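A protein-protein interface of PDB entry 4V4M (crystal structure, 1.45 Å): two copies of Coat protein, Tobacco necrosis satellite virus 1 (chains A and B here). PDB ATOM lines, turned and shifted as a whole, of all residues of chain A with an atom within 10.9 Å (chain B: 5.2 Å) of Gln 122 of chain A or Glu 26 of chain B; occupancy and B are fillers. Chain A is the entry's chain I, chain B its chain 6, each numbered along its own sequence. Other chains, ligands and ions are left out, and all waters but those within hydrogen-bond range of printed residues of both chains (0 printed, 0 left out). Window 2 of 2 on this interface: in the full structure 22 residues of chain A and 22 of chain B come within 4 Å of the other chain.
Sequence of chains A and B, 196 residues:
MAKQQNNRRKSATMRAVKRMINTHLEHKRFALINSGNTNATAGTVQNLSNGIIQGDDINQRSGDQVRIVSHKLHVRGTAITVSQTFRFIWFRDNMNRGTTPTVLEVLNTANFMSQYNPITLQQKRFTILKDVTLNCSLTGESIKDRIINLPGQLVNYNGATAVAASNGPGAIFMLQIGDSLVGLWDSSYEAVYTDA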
ATOM      1  N   ASN A  94      19.080 -11.235 -29.334  1.00  0.00           N
ATOM      2  CA  ASN A  94      20.071 -10.212 -28.986  1.00  0.00           C
ATOM      3  C   ASN A  94      20.785  -9.647 -30.204  1.00  0.00           C
ATOM      4  O   ASN A  94      21.509  -8.651 -30.103  1.00  0.00           O
ATOM      5  CB  ASN A  94      21.132 -10.818 -28.046  1.00  0.00           C
ATOM      6  CG  ASN A  94      20.535 -11.454 -26.793  1.00  0.00           C
ATOM      7  OD1 ASN A  94      20.907 -12.572 -26.399  1.00  0.00           O
ATOM      8  ND2 ASN A  94      19.659 -10.743 -26.141  1.00  0.00           N
ATOM      9  N   MET A  95      20.601 -10.298 -31.352  1.00  0.00           N
ATOM     10  CA  MET A  95      21.437 -10.034 -32.528  1.00  0.00           C
ATOM     11  C   MET A  95      20.616  -9.863 -33.809  1.00  0.00           C
ATOM     12  O   MET A  95      21.128 -10.029 -34.926  1.00  0.00           O
ATOM     13  CB  MET A  95      22.446 -11.182 -32.691  1.00  0.00           C
ATOM     14  CG  MET A  95      23.375 -11.317 -31.503  1.00  0.00           C
ATOM     15  SD  MET A  95      24.655 -12.535 -31.798  1.00  0.00           S
ATOM     16  CE  MET A  95      25.647 -12.400 -30.302  1.00  0.00           C
ATOM     17  N   GLU A 105      16.527 -22.035 -35.563  1.00  0.00           N
ATOM     18  CA  GLU A 105      17.528 -21.164 -34.966  1.00  0.00           C
ATOM     19  C   GLU A 105      17.501 -21.314 -33.455  1.00  0.00           C
ATOM     20  O   GLU A 105      18.542 -21.230 -32.817  1.00  0.00           O
ATOM     21  CB  GLU A 105      17.278 -19.699 -35.317  1.00  0.00           C
ATOM     22  CG  GLU A 105      17.820 -19.285 -36.665  1.00  0.00           C
ATOM     23  CD  GLU A 105      17.639 -17.795 -36.895  1.00  0.00           C
ATOM     24  OE1 GLU A 105      18.509 -17.020 -36.434  1.00  0.00           O
ATOM     25  OE2 GLU A 105      16.625 -17.403 -37.515  1.00  0.00           O
ATOM     26  N   VAL A 106      16.319 -21.562 -32.891  1.00  0.00           N
ATOM     27  CA  VAL A 106      16.169 -21.623 -31.423  1.00  0.00           C
ATOM     28  C   VAL A 106      16.317 -23.049 -30.876  1.00  0.00           C
ATOM     29  O   VAL A 106      16.933 -23.265 -29.815  1.00  0.00           O
ATOM     30  CB  VAL A 106      14.810 -21.026 -30.963  1.00  0.00           C
ATOM     31  CG1 VAL A 106      14.656 -21.108 -29.457  1.00  0.00           C
ATOM     32  CG2 VAL A 106      14.628 -19.588 -31.466  1.00  0.00           C
ATOM     33  N   LEU A 107      15.726 -24.012 -31.591  1.00  0.00           N
ATOM     34  CA  LEU A 107      15.703 -25.409 -31.163  1.00  0.00           C
ATOM     35  C   LEU A 107      16.593 -26.302 -32.018  1.00  0.00           C
ATOM     36  O   LEU A 107      16.692 -26.135 -33.240  1.00  0.00           O
ATOM     37  CB  LEU A 107      14.273 -25.936 -31.261  1.00  0.00           C
ATOM     38  CG  LEU A 107      13.240 -25.335 -30.306  1.00  0.00           C
ATOM     39  CD1 LEU A 107      11.868 -25.992 -30.545  1.00  0.00           C
ATOM     40  CD2 LEU A 107      13.683 -25.584 -28.886  1.00  0.00           C
ATOM     41  N   ASN A 108      17.246 -27.261 -31.378  1.00  0.00           N
ATOM     42  CA  ASN A 108      18.150 -28.130 -32.117  1.00  0.00           C
ATOM     43  C   ASN A 108      17.437 -28.840 -33.280  1.00  0.00           C
ATOM     44  O   ASN A 108      17.936 -28.884 -34.417  1.00  0.00           O
ATOM     45  CB  ASN A 108      18.777 -29.147 -31.172  1.00  0.00           C
ATOM     46  CG  ASN A 108      19.834 -29.968 -31.842  1.00  0.00           C
ATOM     47  OD1 ASN A 108      20.829 -29.431 -32.347  1.00  0.00           O
ATOM     48  ND2 ASN A 108      19.649 -31.277 -31.835  1.00  0.00           N
ATOM     49  N   GLN A 115      15.886 -29.833 -27.132  1.00  0.00           N
ATOM     50  CA  GLN A 115      16.720 -28.891 -26.406  1.00  0.00           C
ATOM     51  C   GLN A 115      17.090 -27.713 -27.323  1.00  0.00           C
ATOM     52  O   GLN A 115      16.790 -27.728 -28.533  1.00  0.00           O
ATOM     53  CB  GLN A 115      17.965 -29.606 -25.878  1.00  0.00           C
ATOM     54  CG  GLN A 115      17.632 -30.774 -24.971  1.00  0.00           C
ATOM     55  CD  GLN A 115      17.297 -30.350 -23.558  1.00  0.00           C
ATOM     56  OE1 GLN A 115      17.766 -29.316 -23.074  1.00  0.00           O
ATOM     57  NE2 GLN A 115      16.482 -31.152 -22.881  1.00  0.00           N
ATOM     58  N   TYR A 116      17.702 -26.673 -26.767  1.00  0.00           N
ATOM     59  CA  TYR A 116      18.038 -25.491 -27.568  1.00  0.00           C
ATOM     60  C   TYR A 116      19.159 -25.804 -28.567  1.00  0.00           C
ATOM     61  O   TYR A 116      19.932 -26.725 -28.372  1.00  0.00           O
ATOM     62  CB  TYR A 116      18.452 -24.313 -26.680  1.00  0.00           C
ATOM     63  CG  TYR A 116      17.431 -23.938 -25.635  1.00  0.00           C
ATOM     64  CD1 TYR A 116      17.813 -23.733 -24.314  1.00  0.00           C
ATOM     65  CD2 TYR A 116      16.081 -23.837 -25.945  1.00  0.00           C
ATOM     66  CE1 TYR A 116      16.882 -23.414 -23.338  1.00  0.00           C
ATOM     67  CE2 TYR A 116      15.143 -23.514 -24.972  1.00  0.00           C
ATOM     68  CZ  TYR A 116      15.552 -23.306 -23.677  1.00  0.00           C
ATOM     69  OH  TYR A 116      14.629 -23.003 -22.699  1.00  0.00           O
ATOM     70  N   ASN A 117      19.223 -25.019 -29.637  1.00  0.00           N
ATOM     71  CA  ASN A 117      20.277 -25.104 -30.633  1.00  0.00           C
ATOM     72  C   ASN A 117      21.619 -24.811 -29.943  1.00  0.00           C
ATOM     73  O   ASN A 117      21.798 -23.733 -29.337  1.00  0.00           O
ATOM     74  CB  ASN A 117      19.927 -24.060 -31.707  1.00  0.00           C
ATOM     75  CG  ASN A 117      20.945 -23.951 -32.824  1.00  0.00           C
ATOM     76  OD1 ASN A 117      22.156 -23.935 -32.595  1.00  0.00           O
ATOM     77  ND2 ASN A 117      20.444 -23.825 -34.057  1.00  0.00           N
ATOM     78  N   PRO A 118      22.556 -25.767 -29.989  1.00  0.00           N
ATOM     79  CA  PRO A 118      23.804 -25.584 -29.274  1.00  0.00           C
ATOM     80  C   PRO A 118      24.591 -24.370 -29.745  1.00  0.00           C
ATOM     81  O   PRO A 118      25.183 -23.676 -28.922  1.00  0.00           O
ATOM     82  CB  PRO A 118      24.581 -26.863 -29.611  1.00  0.00           C
ATOM     83  CG  PRO A 118      23.532 -27.872 -29.818  1.00  0.00           C
ATOM     84  CD  PRO A 118      22.442 -27.136 -30.534  1.00  0.00           C
ATOM     85  N   ILE A 119      24.621 -24.127 -31.054  1.00  0.00           N
ATOM     86  CA  ILE A 119      25.441 -23.041 -31.612  1.00  0.00           C
ATOM     87  C   ILE A 119      24.891 -21.651 -31.273  1.00  0.00           C
ATOM     88  O   ILE A 119      25.632 -20.777 -30.820  1.00  0.00           O
ATOM     89  CB  ILE A 119      25.589 -23.213 -33.139  1.00  0.00           C
ATOM     90  CG1 ILE A 119      26.357 -24.501 -33.430  1.00  0.00           C
ATOM     91  CG2 ILE A 119      26.309 -22.038 -33.731  1.00  0.00           C
ATOM     92  CD1 ILE A 119      26.336 -24.900 -34.890  1.00  0.00           C
ATOM     93  N   THR A 120      23.598 -21.440 -31.479  1.00  0.00           N
ATOM     94  CA  THR A 120      23.035 -20.112 -31.242  1.00  0.00           C
ATOM     95  C   THR A 120      22.985 -19.769 -29.748  1.00  0.00           C
ATOM     96  O   THR A 120      23.054 -18.610 -29.374  1.00  0.00           O
ATOM     97  CB  THR A 120      21.638 -19.944 -31.858  1.00  0.00           C
ATOM     98  OG1 THR A 120      20.753 -20.894 -31.271  1.00  0.00           O
ATOM     99  CG2 THR A 120      21.698 -20.159 -33.347  1.00  0.00           C
ATOM    100  N   LEU A 121      22.859 -20.773 -28.888  1.00  0.00           N
ATOM    101  CA  LEU A 121      22.890 -20.491 -27.459  1.00  0.00           C
ATOM    102  C   LEU A 121      24.344 -20.295 -27.002  1.00  0.00           C
ATOM    103  O   LEU A 121      24.619 -19.433 -26.163  1.00  0.00           O
ATOM    104  CB  LEU A 121      22.186 -21.588 -26.648  1.00  0.00           C
ATOM    105  CG  LEU A 121      20.676 -21.373 -26.431  1.00  0.00           C
ATOM    106  CD1 LEU A 121      20.435 -20.243 -25.406  1.00  0.00           C
ATOM    107  CD2 LEU A 121      19.899 -21.109 -27.738  1.00  0.00           C
ATOM    108  N   GLN A 122      25.279 -21.079 -27.547  1.00  0.00           N
ATOM    109  CA  GLN A 122      26.682 -20.861 -27.178  1.00  0.00           C
ATOM    110  C   GLN A 122      27.109 -19.411 -27.405  1.00  0.00           C
ATOM    111  O   GLN A 122      27.751 -18.797 -26.547  1.00  0.00           O
ATOM    112  CB  GLN A 122      27.643 -21.775 -27.938  1.00  0.00           C
ATOM    113  CG  GLN A 122      29.117 -21.426 -27.660  1.00  0.00           C
ATOM    114  CD  GLN A 122      30.070 -22.201 -28.543  1.00  0.00           C
ATOM    115  OE1 GLN A 122      30.184 -21.923 -29.738  1.00  0.00           O
ATOM    116  NE2 GLN A 122      30.742 -23.197 -27.969  1.00  0.00           N
ATOM    117  N   GLN A 123      26.768 -18.870 -28.572  1.00  0.00           N
ATOM    118  CA  GLN A 123      27.211 -17.536 -28.944  1.00  0.00           C
ATOM    119  C   GLN A 123      26.256 -16.451 -28.411  1.00  0.00           C
ATOM    120  O   GLN A 123      26.449 -15.265 -28.689  1.00  0.00           O
ATOM    121  CB  GLN A 123      27.316 -17.440 -30.472  1.00  0.00           C
ATOM    122  CG  GLN A 123      25.915 -17.434 -31.122  1.00  0.00           C
ATOM    123  CD  GLN A 123      25.917 -17.726 -32.627  1.00  0.00           C
ATOM    124  OE1 GLN A 123      25.081 -17.205 -33.353  1.00  0.00           O
ATOM    125  NE2 GLN A 123      26.847 -18.554 -33.088  1.00  0.00           N
ATOM    126  N   LYS A 124      25.222 -16.867 -27.673  1.00  0.00           N
ATOM    127  CA  LYS A 124      24.256 -15.935 -27.041  1.00  0.00           C
ATOM    128  C   LYS A 124      23.487 -15.093 -28.050  1.00  0.00           C
ATOM    129  O   LYS A 124      23.132 -13.932 -27.805  1.00  0.00           O
ATOM    130  CB  LYS A 124      24.945 -15.060 -25.981  1.00  0.00           C
ATOM    131  CG  LYS A 124      25.565 -15.900 -24.847  1.00  0.00           C
ATOM    132  CD  LYS A 124      25.994 -15.057 -23.664  1.00  0.00           C
ATOM    133  CE  LYS A 124      26.414 -15.963 -22.509  1.00  0.00           C
ATOM    134  NZ  LYS A 124      27.429 -16.933 -22.984  1.00  0.00           N
ATOM    135  N   ARG A 125      23.188 -15.704 -29.186  1.00  0.00           N
ATOM    136  CA  ARG A 125      22.306 -15.060 -30.156  1.00  0.00           C
ATOM    137  C   ARG A 125      20.930 -14.793 -29.533  1.00  0.00           C
ATOM    138  O   ARG A 125      20.276 -13.792 -29.836  1.00  0.00           O
ATOM    139  CB  ARG A 125      22.148 -15.953 -31.383  1.00  0.00           C
ATOM    140  CG  ARG A 125      21.434 -15.238 -32.535  1.00  0.00           C
ATOM    141  CD  ARG A 125      21.162 -16.167 -33.722  1.00  0.00           C
ATOM    142  NE  ARG A 125      22.391 -16.709 -34.296  1.00  0.00           N
ATOM    143  CZ  ARG A 125      22.431 -17.395 -35.438  1.00  0.00           C
ATOM    144  NH1 ARG A 125      23.584 -17.892 -35.873  1.00  0.00           N
ATOM    145  NH2 ARG A 125      21.315 -17.608 -36.136  1.00  0.00           N
ATOM    146  N   PHE A 126      20.485 -15.715 -28.682  1.00  0.00           N
ATOM    147  CA  PHE A 126      19.182 -15.606 -28.029  1.00  0.00           C
ATOM    148  C   PHE A 126      19.370 -15.719 -26.532  1.00  0.00           C
ATOM    149  O   PHE A 126      20.288 -16.386 -26.077  1.00  0.00           O
ATOM    150  CB  PHE A 126      18.259 -16.758 -28.466  1.00  0.00           C
ATOM    151  CG  PHE A 126      18.061 -16.839 -29.954  1.00  0.00           C
ATOM    152  CD1 PHE A 126      18.555 -17.918 -30.675  1.00  0.00           C
ATOM    153  CD2 PHE A 126      17.388 -15.832 -30.625  1.00  0.00           C
ATOM    154  CE1 PHE A 126      18.391 -17.984 -32.060  1.00  0.00           C
ATOM    155  CE2 PHE A 126      17.211 -15.875 -32.021  1.00  0.00           C
ATOM    156  CZ  PHE A 126      17.701 -16.962 -32.735  1.00  0.00           C
ATOM    157  N   THR A 127      18.510 -15.027 -25.786  1.00  0.00           N
ATOM    158  CA  THR A 127      18.362 -15.227 -24.355  1.00  0.00           C
ATOM    159  C   THR A 127      16.945 -15.735 -24.126  1.00  0.00           C
ATOM    160  O   THR A 127      15.964 -15.105 -24.538  1.00  0.00           O
ATOM    161  CB  THR A 127      18.566 -13.916 -23.580  1.00  0.00           C
ATOM    162  OG1 THR A 127      19.892 -13.421 -23.826  1.00  0.00           O
ATOM    163  CG2 THR A 127      18.353 -14.132 -22.053  1.00  0.00           C
ATOM    164  N   ILE A 128      16.835 -16.883 -23.467  1.00  0.00           N
ATOM    165  CA  ILE A 128      15.537 -17.476 -23.227  1.00  0.00           C
ATOM    166  C   ILE A 128      14.955 -16.854 -21.966  1.00  0.00           C
ATOM    167  O   ILE A 128      15.585 -16.905 -20.912  1.00  0.00           O
ATOM    168  CB  ILE A 128      15.627 -19.020 -23.058  1.00  0.00           C
ATOM    169  CG1 ILE A 128      16.375 -19.681 -24.227  1.00  0.00           C
ATOM    170  CG2 ILE A 128      14.224 -19.612 -22.860  1.00  0.00           C
ATOM    171  CD1 ILE A 128      15.665 -19.540 -25.573  1.00  0.00           C
ATOM    172  N   HIS B  24      37.960 -18.334 -20.344  1.00  0.00           N
ATOM    173  CA  HIS B  24      38.940 -18.658 -21.374  1.00  0.00           C
ATOM    174  C   HIS B  24      38.650 -20.005 -22.020  1.00  0.00           C
ATOM    175  O   HIS B  24      39.297 -20.388 -22.994  1.00  0.00           O
ATOM    176  CB  HIS B  24      40.349 -18.647 -20.780  1.00  0.00           C
ATOM    177  CG  HIS B  24      40.860 -17.274 -20.478  1.00  0.00           C
ATOM    178  ND1 HIS B  24      41.436 -16.470 -21.437  1.00  0.00           N
ATOM    179  CD2 HIS B  24      40.868 -16.555 -19.329  1.00  0.00           C
ATOM    180  CE1 HIS B  24      41.785 -15.317 -20.893  1.00  0.00           C
ATOM    181  NE2 HIS B  24      41.454 -15.344 -19.613  1.00  0.00           N
ATOM    182  N   LEU B  25      37.680 -20.727 -21.478  1.00  0.00           N
ATOM    183  CA  LEU B  25      37.358 -22.054 -21.985  1.00  0.00           C
ATOM    184  C   LEU B  25      36.074 -22.060 -22.814  1.00  0.00           C
ATOM    185  O   LEU B  25      35.035 -21.552 -22.387  1.00  0.00           O
ATOM    186  CB  LEU B  25      37.237 -23.058 -20.834  1.00  0.00           C
ATOM    187  CG  LEU B  25      38.365 -23.079 -19.804  1.00  0.00           C
ATOM    188  CD1 LEU B  25      38.133 -24.228 -18.844  1.00  0.00           C
ATOM    189  CD2 LEU B  25      39.743 -23.185 -20.444  1.00  0.00           C
ATOM    190  N   GLU B  26      36.141 -22.630 -24.013  1.00  0.00           N
ATOM    191  CA  GLU B  26      34.924 -22.805 -24.783  1.00  0.00           C
ATOM    192  C   GLU B  26      33.923 -23.706 -24.051  1.00  0.00           C
ATOM    193  O   GLU B  26      34.240 -24.831 -23.641  1.00  0.00           O
ATOM    194  CB  GLU B  26      35.204 -23.352 -26.188  1.00  0.00           C
ATOM    195  CG  GLU B  26      33.926 -23.643 -26.975  1.00  0.00           C
ATOM    196  CD  GLU B  26      34.160 -23.923 -28.457  1.00  0.00           C
ATOM    197  OE1 GLU B  26      35.294 -23.744 -28.957  1.00  0.00           O
ATOM    198  OE2 GLU B  26      33.182 -24.314 -29.122  1.00  0.00           O
ATOM    199  N   HIS B  27      32.714 -23.200 -23.877  1.00  0.00           N
ATOM    200  CA  HIS B  27      31.629 -24.054 -23.399  1.00  0.00           C
ATOM    201  C   HIS B  27      30.960 -24.723 -24.595  1.00  0.00           C
ATOM    202  O   HIS B  27      30.057 -24.173 -25.241  1.00  0.00           O
ATOM    203  CB  HIS B  27      30.672 -23.281 -22.493  1.00  0.00           C
ATOM    204  CG  HIS B  27      31.318 -22.821 -21.224  1.00  0.00           C
ATOM    205  ND1 HIS B  27      30.727 -22.963 -19.986  1.00  0.00           N
ATOM    206  CD2 HIS B  27      32.523 -22.246 -21.003  1.00  0.00           C
ATOM    207  CE1 HIS B  27      31.532 -22.472 -19.057  1.00  0.00           C
ATOM    208  NE2 HIS B  27      32.626 -22.030 -19.647  1.00  0.00           N
ATOM    209  N   LYS B  28      31.474 -25.906 -24.912  1.00  0.00           N
ATOM    210  CA  LYS B  28      30.910 -26.751 -25.950  1.00  0.00           C
ATOM    211  C   LYS B  28      29.533 -27.224 -25.497  1.00  0.00           C
ATOM    212  O   LYS B  28      29.152 -27.126 -24.314  1.00  0.00           O
ATOM    213  CB  LYS B  28      31.860 -27.913 -26.259  1.00  0.00           C
ATOM    214  CG  LYS B  28      33.159 -27.447 -26.929  1.00  0.00           C
ATOM    215  CD  LYS B  28      34.007 -28.621 -27.413  1.00  0.00           C
ATOM    216  CE  LYS B  28      35.295 -28.114 -28.070  1.00  0.00           C
ATOM    217  NZ  LYS B  28      36.256 -29.220 -28.414  1.00  0.00           N
ATOM    218  N   ARG B  29      28.741 -27.697 -26.445  1.00  0.00           N
ATOM    219  CA  ARG B  29      27.343 -28.026 -26.147  1.00  0.00           C
ATOM    220  C   ARG B  29      26.843 -29.151 -27.025  1.00  0.00           C
ATOM    221  O   ARG B  29      27.047 -29.115 -28.246  1.00  0.00           O
ATOM    222  CB  ARG B  29      26.444 -26.808 -26.347  1.00  0.00           C
ATOM    223  CG  ARG B  29      26.588 -25.738 -25.305  1.00  0.00           C
ATOM    224  CD  ARG B  29      25.701 -24.558 -25.654  1.00  0.00           C
ATOM    225  NE  ARG B  29      24.310 -24.745 -25.255  1.00  0.00           N
ATOM    226  CZ  ARG B  29      23.712 -24.037 -24.301  1.00  0.00           C
ATOM    227  NH1 ARG B  29      24.395 -23.113 -23.641  1.00  0.00           N
ATOM    228  NH2 ARG B  29      22.446 -24.266 -24.002  1.00  0.00           N
ATOM    229  N   ILE B  58      31.342 -28.460 -32.319  1.00  0.00           N
ATOM    230  CA  ILE B  58      30.877 -27.866 -31.078  1.00  0.00           C
ATOM    231  C   ILE B  58      30.333 -28.899 -30.108  1.00  0.00           C
ATOM    232  O   ILE B  58      30.322 -28.671 -28.910  1.00  0.00           O
ATOM    233  CB  ILE B  58      29.806 -26.777 -31.327  1.00  0.00           C
ATOM    234  CG1 ILE B  58      29.422 -26.068 -30.029  1.00  0.00           C
ATOM    235  CG2 ILE B  58      28.545 -27.376 -31.976  1.00  0.00           C
ATOM    236  CD1 ILE B  58      28.509 -24.885 -30.274  1.00  0.00           C
ATOM    237  N   TYR B 193      29.580 -28.200 -21.664  1.00  0.00           N
ATOM    238  CA  TYR B 193      30.815 -28.757 -21.094  1.00  0.00           C
ATOM    239  C   TYR B 193      32.052 -28.023 -21.588  1.00  0.00           C
ATOM    240  O   TYR B 193      32.063 -27.461 -22.689  1.00  0.00           O
ATOM    241  CB  TYR B 193      30.929 -30.256 -21.417  1.00  0.00           C
ATOM    242  CG  TYR B 193      30.931 -30.591 -22.904  1.00  0.00           C
ATOM    243  CD1 TYR B 193      29.732 -30.684 -23.618  1.00  0.00           C
ATOM    244  CD2 TYR B 193      32.122 -30.827 -23.592  1.00  0.00           C
ATOM    245  CE1 TYR B 193      29.723 -30.986 -24.983  1.00  0.00           C
ATOM    246  CE2 TYR B 193      32.118 -31.128 -24.964  1.00  0.00           C
ATOM    247  CZ  TYR B 193      30.906 -31.220 -25.651  1.00  0.00           C
ATOM    248  OH  TYR B 193      30.854 -31.531 -27.023  1.00  0.00           O
ATOM    249  N   THR B 194      33.097 -28.015 -20.772  1.00  0.00           N
ATOM    250  CA  THR B 194      34.392 -27.547 -21.224  1.00  0.00           C
ATOM    251  C   THR B 194      35.227 -28.748 -21.651  1.00  0.00           C
ATOM    252  O   THR B 194      34.980 -29.889 -21.230  1.00  0.00           O
ATOM    253  CB  THR B 194      35.145 -26.739 -20.140  1.00  0.00           C
ATOM    254  OG1 THR B 194      35.401 -27.571 -18.987  1.00  0.00           O
ATOM    255  CG2 THR B 194      34.337 -25.509 -19.743  1.00  0.00           C
ATOM    256  N   ASP B 195      36.240 -28.476 -22.462  1.00  0.00           N
ATOM    257  CA  ASP B 195      37.034 -29.519 -23.089  1.00  0.00           C
ATOM    258  C   ASP B 195      38.469 -29.028 -23.254  1.00  0.00           C
ATOM    259  O   ASP B 195      39.040 -29.132 -24.338  1.00  0.00           O
ATOM    260  CB  ASP B 195      36.409 -29.833 -24.446  1.00  0.00           C
ATOM    261  CG  ASP B 195      37.068 -30.995 -25.146  1.00  0.00           C
ATOM    262  OD1 ASP B 195      37.068 -30.999 -26.398  1.00  0.00           O
ATOM    263  OD2 ASP B 195      37.576 -31.910 -24.464  1.00  0.00           O
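N of Arg 29 of chain B lies within hydrogen-bond range of O of Ile 58 of chain B (3.1 Å).
The side-chain hydroxyl (OH) of Tyr 193 of chain B lies within hydrogen-bond range of the backbone carbonyl oxygen (O) of Ile 58 of chain B.
OD1 of Asn 117 of chain A sits at hydrogen-bond distance from N of Ile 119 of chain A (2.9 Å).
The side-chain amide nitrogen (NE2) of Gln 123 of chain A lies close to the backbone carbonyl oxygen (O) of Ile 119 of chain A (3.4 Å).
OE2 of Glu 26 of chain B is in hydrogen-bond range of NE2 of Gln 122 of chain A (2.9 Å).
The backbone carbonyl oxygen (O) of His 27 of chain B is in hydrogen-bond range of the side-chain amide nitrogen (NE2) of Gln 122 of chain A (3.0 Å).
Along chain A the printed residues that touch a printed residue of chain B span positions 118 to 122.
Of the 10 printed residues of chain B, 4 touch a printed residue of chain A.
Among the printed residues, 8 pairs touch across the chains.
Printed residues of chain B within 4 Å of Gln 122 of chain A: Glu 26, His 27, Arg 29 and Ile 58.
Glu 26 of chain B touches one residue of chain A.
No residue of chain A comes within 4 Å of Leu 25 of chain B.
Of chain A, only Gln 122 comes within 4 Å of His 27 of chain B.
No residue of chain A comes within 4 Å of Lys 28 of chain B.
Of the printed residues of chain A, Ile 58 of chain B touches Pro 118, Ile 119 and Gln 122.
No residue of chain A comes within 4 Å of Thr 194 of chain B.
Printed residues of chain B within 4 Å of Leu 121 of chain A: Arg 29 (3.7 Å).
Of the printed residues of chain B, Ile 119 of chain A touches Ile 58 (3.8 Å).
The nearest printed residue of chain B that does not touch Gln 122 of chain A is Lys 28 of chain B (4.1 Å).
The nearest printed residue of chain B that does not touch Pro 118 of chain A is His 27 of chain B (6.1 Å).
Among the printed residues, pairs that only touch across the chains: Pro 118 of chain A with Arg 29 of chain B (3.4 Å), Gln 122 of chain A with Ile 58 of chain B (3.4 Å), Leu 121 of chain A with Arg 29 of chain B (3.7 Å), Pro 118 of chain A with Ile 58 of chain B (3.8 Å), Ile 119 of chain A with Ile 58 of chain B (3.8 Å) and Gln 122 of chain A with Arg 29 of chain B (3.98 Å).
No position is printed for both chains.
Of the 8 pairs that touch across the chains among the printed residues, none has its exchanged pair printed and touching as well.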
